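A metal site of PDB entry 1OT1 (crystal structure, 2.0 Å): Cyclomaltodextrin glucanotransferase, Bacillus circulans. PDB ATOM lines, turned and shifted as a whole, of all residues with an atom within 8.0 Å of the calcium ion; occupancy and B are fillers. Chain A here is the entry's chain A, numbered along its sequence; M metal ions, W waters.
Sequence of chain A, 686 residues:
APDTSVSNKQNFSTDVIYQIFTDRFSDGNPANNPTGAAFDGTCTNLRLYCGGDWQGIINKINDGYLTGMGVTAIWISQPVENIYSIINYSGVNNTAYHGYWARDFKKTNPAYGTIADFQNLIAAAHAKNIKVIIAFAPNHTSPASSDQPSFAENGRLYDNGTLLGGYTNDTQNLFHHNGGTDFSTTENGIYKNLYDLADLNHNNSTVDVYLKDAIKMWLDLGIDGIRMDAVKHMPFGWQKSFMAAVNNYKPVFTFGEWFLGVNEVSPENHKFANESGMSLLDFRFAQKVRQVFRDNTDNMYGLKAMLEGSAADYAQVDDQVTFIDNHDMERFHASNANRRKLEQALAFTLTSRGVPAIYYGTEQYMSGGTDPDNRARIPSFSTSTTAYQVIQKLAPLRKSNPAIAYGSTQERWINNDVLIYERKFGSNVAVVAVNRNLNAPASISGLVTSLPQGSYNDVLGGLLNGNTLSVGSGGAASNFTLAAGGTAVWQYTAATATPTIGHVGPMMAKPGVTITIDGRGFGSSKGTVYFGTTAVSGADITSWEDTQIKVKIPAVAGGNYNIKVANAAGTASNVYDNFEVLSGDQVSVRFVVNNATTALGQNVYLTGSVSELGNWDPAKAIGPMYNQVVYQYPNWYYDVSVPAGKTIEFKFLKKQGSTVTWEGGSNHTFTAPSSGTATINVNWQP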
ATOM      1  N   THR A  22       4.156   4.978  -8.825  1.00  0.00           N
ATOM      2  CA  THR A  22       3.541   5.721  -7.730  1.00  0.00           C
ATOM      3  C   THR A  22       3.610   5.168  -6.311  1.00  0.00           C
ATOM      4  O   THR A  22       4.022   5.874  -5.389  1.00  0.00           O
ATOM      5  CB  THR A  22       2.069   6.035  -8.049  1.00  0.00           C
ATOM      6  OG1 THR A  22       1.993   6.605  -9.359  1.00  0.00           O
ATOM      7  CG2 THR A  22       1.507   7.027  -7.044  1.00  0.00           C
ATOM      8  N   ASP A  23       3.205   3.916  -6.113  1.00  0.00           N
ATOM      9  CA  ASP A  23       3.193   3.352  -4.770  1.00  0.00           C
ATOM     10  C   ASP A  23       4.585   3.234  -4.149  1.00  0.00           C
ATOM     11  O   ASP A  23       4.723   3.198  -2.916  1.00  0.00           O
ATOM     12  CB  ASP A  23       2.530   1.978  -4.765  1.00  0.00           C
ATOM     13  CG  ASP A  23       2.359   1.423  -3.363  1.00  0.00           C
ATOM     14  OD1 ASP A  23       1.627   2.044  -2.565  1.00  0.00           O
ATOM     15  OD2 ASP A  23       2.971   0.372  -3.052  1.00  0.00           O
ATOM     16  N   SER A  26       6.942   8.031  -3.309  1.00  0.00           N
ATOM     17  CA  SER A  26       6.863   8.804  -2.078  1.00  0.00           C
ATOM     18  C   SER A  26       5.460   8.910  -1.485  1.00  0.00           C
ATOM     19  O   SER A  26       4.529   9.383  -2.132  1.00  0.00           O
ATOM     20  CB  SER A  26       7.409  10.222  -2.313  1.00  0.00           C
ATOM     21  OG  SER A  26       7.418  10.964  -1.098  1.00  0.00           O
ATOM     22  N   ASP A  27       5.333   8.461  -0.236  1.00  0.00           N
ATOM     23  CA  ASP A  27       4.068   8.507   0.480  1.00  0.00           C
ATOM     24  C   ASP A  27       3.927   9.896   1.109  1.00  0.00           C
ATOM     25  O   ASP A  27       4.409  10.134   2.214  1.00  0.00           O
ATOM     26  CB  ASP A  27       4.042   7.417   1.568  1.00  0.00           C
ATOM     27  CG  ASP A  27       2.778   7.436   2.416  1.00  0.00           C
ATOM     28  OD1 ASP A  27       1.809   8.142   2.043  1.00  0.00           O
ATOM     29  OD2 ASP A  27       2.751   6.734   3.444  1.00  0.00           O
ATOM     30  N   GLY A  28       3.299  10.802   0.380  1.00  0.00           N
ATOM     31  CA  GLY A  28       3.132  12.170   0.867  1.00  0.00           C
ATOM     32  C   GLY A  28       1.920  12.355   1.744  1.00  0.00           C
ATOM     33  O   GLY A  28       1.779  13.380   2.416  1.00  0.00           O
ATOM     34  N   ASN A  29       1.012  11.372   1.741  1.00  0.00           N
ATOM     35  CA  ASN A  29      -0.196  11.430   2.562  1.00  0.00           C
ATOM     36  C   ASN A  29      -0.511  10.075   3.173  1.00  0.00           C
ATOM     37  O   ASN A  29      -1.166   9.236   2.563  1.00  0.00           O
ATOM     38  CB  ASN A  29      -1.384  11.903   1.707  1.00  0.00           C
ATOM     39  CG  ASN A  29      -2.678  11.993   2.502  1.00  0.00           C
ATOM     40  OD1 ASN A  29      -2.672  11.828   3.720  1.00  0.00           O
ATOM     41  ND2 ASN A  29      -3.778  12.269   1.815  1.00  0.00           N
ATOM     42  N   PRO A  30      -0.041   9.841   4.405  1.00  0.00           N
ATOM     43  CA  PRO A  30      -0.274   8.567   5.103  1.00  0.00           C
ATOM     44  C   PRO A  30      -1.763   8.264   5.297  1.00  0.00           C
ATOM     45  O   PRO A  30      -2.156   7.109   5.425  1.00  0.00           O
ATOM     46  CB  PRO A  30       0.447   8.757   6.428  1.00  0.00           C
ATOM     47  CG  PRO A  30       1.546   9.723   6.095  1.00  0.00           C
ATOM     48  CD  PRO A  30       0.829  10.718   5.208  1.00  0.00           C
ATOM     49  N   ALA A  31      -2.571   9.322   5.313  1.00  0.00           N
ATOM     50  CA  ALA A  31      -4.015   9.188   5.524  1.00  0.00           C
ATOM     51  C   ALA A  31      -4.745   8.372   4.453  1.00  0.00           C
ATOM     52  O   ALA A  31      -5.764   7.738   4.748  1.00  0.00           O
ATOM     53  CB  ALA A  31      -4.653  10.570   5.658  1.00  0.00           C
ATOM     54  N   ASN A  32      -4.250   8.388   3.223  1.00  0.00           N
ATOM     55  CA  ASN A  32      -4.913   7.622   2.163  1.00  0.00           C
ATOM     56  C   ASN A  32      -4.329   6.226   1.987  1.00  0.00           C
ATOM     57  O   ASN A  32      -4.690   5.512   1.050  1.00  0.00           O
ATOM     58  CB  ASN A  32      -4.857   8.366   0.823  1.00  0.00           C
ATOM     59  CG  ASN A  32      -3.442   8.635   0.351  1.00  0.00           C
ATOM     60  OD1 ASN A  32      -2.531   7.842   0.589  1.00  0.00           O
ATOM     61  ND2 ASN A  32      -3.256   9.759  -0.349  1.00  0.00           N
ATOM     62  N   ASN A  33      -3.424   5.830   2.871  1.00  0.00           N
ATOM     63  CA  ASN A  33      -2.821   4.504   2.781  1.00  0.00           C
ATOM     64  C   ASN A  33      -3.827   3.391   3.028  1.00  0.00           C
ATOM     65  O   ASN A  33      -4.679   3.491   3.906  1.00  0.00           O
ATOM     66  CB  ASN A  33      -1.683   4.348   3.790  1.00  0.00           C
ATOM     67  CG  ASN A  33      -0.503   5.231   3.487  1.00  0.00           C
ATOM     68  OD1 ASN A  33      -0.441   5.866   2.430  1.00  0.00           O
ATOM     69  ND2 ASN A  33       0.457   5.275   4.404  1.00  0.00           N
ATOM     70  N   PRO A  34      -3.760   2.308   2.221  1.00  0.00           N
ATOM     71  CA  PRO A  34      -4.678   1.190   2.435  1.00  0.00           C
ATOM     72  C   PRO A  34      -4.330   0.618   3.818  1.00  0.00           C
ATOM     73  O   PRO A  34      -3.257   0.901   4.350  1.00  0.00           O
ATOM     74  CB  PRO A  34      -4.317   0.234   1.310  1.00  0.00           C
ATOM     75  CG  PRO A  34      -3.932   1.179   0.198  1.00  0.00           C
ATOM     76  CD  PRO A  34      -3.059   2.174   0.925  1.00  0.00           C
ATOM     77  N   PHE A  39      -1.649  -3.668   3.182  1.00  0.00           N
ATOM     78  CA  PHE A  39      -0.626  -2.654   3.372  1.00  0.00           C
ATOM     79  C   PHE A  39       0.592  -3.096   4.178  1.00  0.00           C
ATOM     80  O   PHE A  39       0.496  -3.875   5.129  1.00  0.00           O
ATOM     81  CB  PHE A  39      -1.263  -1.443   4.057  1.00  0.00           C
ATOM     82  CG  PHE A  39      -0.320  -0.284   4.251  1.00  0.00           C
ATOM     83  CD1 PHE A  39       0.045   0.504   3.161  1.00  0.00           C
ATOM     84  CD2 PHE A  39       0.184   0.021   5.506  1.00  0.00           C
ATOM     85  CE1 PHE A  39       0.908   1.595   3.338  1.00  0.00           C
ATOM     86  CE2 PHE A  39       1.047   1.098   5.686  1.00  0.00           C
ATOM     87  CZ  PHE A  39       1.406   1.880   4.598  1.00  0.00           C
ATOM     88  N   TYR A  49       0.458  -2.706  -0.885  1.00  0.00           N
ATOM     89  CA  TYR A  49       0.604  -1.264  -1.001  1.00  0.00           C
ATOM     90  C   TYR A  49       1.644  -0.791   0.005  1.00  0.00           C
ATOM     91  O   TYR A  49       1.666  -1.249   1.153  1.00  0.00           O
ATOM     92  CB  TYR A  49      -0.722  -0.551  -0.715  1.00  0.00           C
ATOM     93  CG  TYR A  49      -1.670  -0.442  -1.894  1.00  0.00           C
ATOM     94  CD1 TYR A  49      -2.620  -1.427  -2.150  1.00  0.00           C
ATOM     95  CD2 TYR A  49      -1.632   0.678  -2.729  1.00  0.00           C
ATOM     96  CE1 TYR A  49      -3.541  -1.288  -3.200  1.00  0.00           C
ATOM     97  CE2 TYR A  49      -2.539   0.819  -3.779  1.00  0.00           C
ATOM     98  CZ  TYR A  49      -3.491  -0.157  -4.006  1.00  0.00           C
ATOM     99  OH  TYR A  49      -4.394  -0.001  -5.029  1.00  0.00           O
ATOM    100  N   CYS A  50       2.489   0.126  -0.427  1.00  0.00           N
ATOM    101  CA  CYS A  50       3.533   0.674   0.433  1.00  0.00           C
ATOM    102  C   CYS A  50       3.195   2.103   0.857  1.00  0.00           C
ATOM    103  O   CYS A  50       3.780   2.639   1.801  1.00  0.00           O
ATOM    104  CB  CYS A  50       4.883   0.617  -0.283  1.00  0.00           C
ATOM    105  SG  CYS A  50       5.482  -1.088  -0.483  1.00  0.00           S
ATOM    106  N   GLY A  51       2.251   2.726   0.145  1.00  0.00           N
ATOM    107  CA  GLY A  51       1.830   4.066   0.506  1.00  0.00           C
ATOM    108  C   GLY A  51       2.138   5.199  -0.459  1.00  0.00           C
ATOM    109  O   GLY A  51       1.629   6.306  -0.276  1.00  0.00           O
ATOM    110  N   GLY A  52       2.965   4.941  -1.469  1.00  0.00           N
ATOM    111  CA  GLY A  52       3.319   5.993  -2.417  1.00  0.00           C
ATOM    112  C   GLY A  52       2.088   6.605  -3.065  1.00  0.00           C
ATOM    113  O   GLY A  52       1.210   5.883  -3.517  1.00  0.00           O
ATOM    114  N   ASP A  53       2.049   7.925  -3.139  1.00  0.00           N
ATOM    115  CA  ASP A  53       0.878   8.613  -3.689  1.00  0.00           C
ATOM    116  C   ASP A  53       1.209   9.875  -4.470  1.00  0.00           C
ATOM    117  O   ASP A  53       2.381  10.229  -4.641  1.00  0.00           O
ATOM    118  CB  ASP A  53      -0.110   8.951  -2.558  1.00  0.00           C
ATOM    119  CG  ASP A  53       0.565   9.658  -1.396  1.00  0.00           C
ATOM    120  OD1 ASP A  53       1.417  10.526  -1.647  1.00  0.00           O
ATOM    121  OD2 ASP A  53       0.227   9.359  -0.228  1.00  0.00           O
ATOM    122  N   TRP A  54       0.168  10.574  -4.931  1.00  0.00           N
ATOM    123  CA  TRP A  54       0.367  11.794  -5.709  1.00  0.00           C
ATOM    124  C   TRP A  54       0.874  12.958  -4.871  1.00  0.00           C
ATOM    125  O   TRP A  54       1.600  13.804  -5.376  1.00  0.00           O
ATOM    126  CB  TRP A  54      -0.930  12.175  -6.431  1.00  0.00           C
ATOM    127  CG  TRP A  54      -1.365  11.127  -7.433  1.00  0.00           C
ATOM    128  CD1 TRP A  54      -0.546  10.283  -8.127  1.00  0.00           C
ATOM    129  CD2 TRP A  54      -2.706  10.830  -7.845  1.00  0.00           C
ATOM    130  NE1 TRP A  54      -1.291   9.480  -8.953  1.00  0.00           N
ATOM    131  CE2 TRP A  54      -2.619   9.792  -8.800  1.00  0.00           C
ATOM    132  CE3 TRP A  54      -3.958  11.335  -7.503  1.00  0.00           C
ATOM    133  CZ2 TRP A  54      -3.755   9.245  -9.417  1.00  0.00           C
ATOM    134  CZ3 TRP A  54      -5.094  10.788  -8.119  1.00  0.00           C
ATOM    135  CH2 TRP A  54      -4.973   9.762  -9.065  1.00  0.00           C
ATOM    136  N   GLN A  55       0.507  13.013  -3.599  1.00  0.00           N
ATOM    137  CA  GLN A  55       1.013  14.086  -2.746  1.00  0.00           C
ATOM    138  C   GLN A  55       2.530  13.949  -2.684  1.00  0.00           C
ATOM    139  O   GLN A  55       3.261  14.940  -2.698  1.00  0.00           O
ATOM    140  CB  GLN A  55       0.419  14.008  -1.337  1.00  0.00           C
ATOM    141  CG  GLN A  55       0.890  15.139  -0.430  1.00  0.00           C
ATOM    142  CD  GLN A  55       0.549  16.505  -1.000  1.00  0.00           C
ATOM    143  OE1 GLN A  55      -0.606  16.814  -1.261  1.00  0.00           O
ATOM    144  NE2 GLN A  55       1.570  17.338  -1.196  1.00  0.00           N
ATOM    145  N   GLY A  56       2.998  12.713  -2.623  1.00  0.00           N
ATOM    146  CA  GLY A  56       4.424  12.461  -2.587  1.00  0.00           C
ATOM    147  C   GLY A  56       5.114  12.986  -3.826  1.00  0.00           C
ATOM    148  O   GLY A  56       6.168  13.615  -3.741  1.00  0.00           O
ATOM    149  N   PRO A 110      -8.126   5.794  -4.860  1.00  0.00           N
ATOM    150  CA  PRO A 110      -8.013   6.548  -3.598  1.00  0.00           C
ATOM    151  C   PRO A 110      -6.676   6.420  -2.874  1.00  0.00           C
ATOM    152  O   PRO A 110      -6.296   7.313  -2.113  1.00  0.00           O
ATOM    153  CB  PRO A 110      -9.189   6.012  -2.769  1.00  0.00           C
ATOM    154  CG  PRO A 110      -9.374   4.629  -3.299  1.00  0.00           C
ATOM    155  CD  PRO A 110      -9.224   4.825  -4.786  1.00  0.00           C
ATOM    156  N   ALA A 111      -5.966   5.321  -3.116  1.00  0.00           N
ATOM    157  CA  ALA A 111      -4.655   5.137  -2.503  1.00  0.00           C
ATOM    158  C   ALA A 111      -3.677   6.183  -3.047  1.00  0.00           C
ATOM    159  O   ALA A 111      -2.837   6.700  -2.308  1.00  0.00           O
ATOM    160  CB  ALA A 111      -4.143   3.731  -2.776  1.00  0.00           C
ATOM    161  N   TYR A 112      -3.794   6.491  -4.336  1.00  0.00           N
ATOM    162  CA  TYR A 112      -2.923   7.496  -4.949  1.00  0.00           C
ATOM    163  C   TYR A 112      -3.438   8.892  -4.611  1.00  0.00           C
ATOM    164  O   TYR A 112      -2.653   9.814  -4.392  1.00  0.00           O
ATOM    165  CB  TYR A 112      -2.883   7.345  -6.468  1.00  0.00           C
ATOM    166  CG  TYR A 112      -2.411   6.004  -6.992  1.00  0.00           C
ATOM    167  CD1 TYR A 112      -1.662   5.139  -6.192  1.00  0.00           C
ATOM    168  CD2 TYR A 112      -2.716   5.613  -8.290  1.00  0.00           C
ATOM    169  CE1 TYR A 112      -1.226   3.907  -6.688  1.00  0.00           C
ATOM    170  CE2 TYR A 112      -2.280   4.392  -8.800  1.00  0.00           C
ATOM    171  CZ  TYR A 112      -1.533   3.544  -7.995  1.00  0.00           C
ATOM    172  OH  TYR A 112      -1.127   2.337  -8.500  1.00  0.00           O
ATOM    173  N   GLY A 113      -4.763   9.037  -4.577  1.00  0.00           N
ATOM    174  CA  GLY A 113      -5.348  10.328  -4.256  1.00  0.00           C
ATOM    175  C   GLY A 113      -6.742  10.530  -4.817  1.00  0.00           C
ATOM    176  O   GLY A 113      -7.330   9.650  -5.452  1.00  0.00           O
HETATM  177 CA    CA M   1      -0.273   7.501   0.964  1.00  0.00          CA
HETATM  178  O   HOH W   1      -1.255   5.637  -0.343  1.00  0.00           O
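The side-chain amide nitrogen of Asn 33 sits close to the backbone carbonyl oxygen of Pro 30, at 3.4 Å.
OD1 of Asp 53 sits at hydrogen-bond distance from N of Gly 28 (2.8 Å).
N of Asp 53 sits at hydrogen-bond distance from O of Ser 26, at 3.0 Å.
The side-chain carboxylate (OD1) of Asp 53 lies within hydrogen-bond range of the backbone NH (N) of Gln 55 (3.3 Å).
OD1 of Asp 53 sits at hydrogen-bond distance from N of Gly 56 (2.9 Å).
The side-chain amide oxygen of Asn 32 sits close to the backbone carbonyl oxygen of Ala 111 (3.1 Å).
The side-chain amide oxygen of Asn 29 is in hydrogen-bond range of the backbone NH of Ala 31 (3.0 Å).
N of Gly 51 lies within hydrogen-bond range of OD1 of Asp 23 (2.9 Å).
Within 4 Å of the calcium ion: Asp 27, Asn 29, Asn 32, Asn 33, Gly 51 and Asp 53.
The calcium ion is bound by OD1 of Asn 33 (2.2 Å).
The side-chain carboxylate (OD2) of Asp 53 is bound to the calcium ion.
OD1 of Asn 32 binds the calcium ion (2.3 Å).
OD1 of Asp 27 binds the calcium ion, 2.4 Å away.
The calcium ion is bound by water W1, 2.5 Å away.
The backbone carbonyl oxygen (O) of Asn 29 binds the calcium ion (2.5 Å).
O of Gly 51 binds the calcium ion (2.6 Å).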
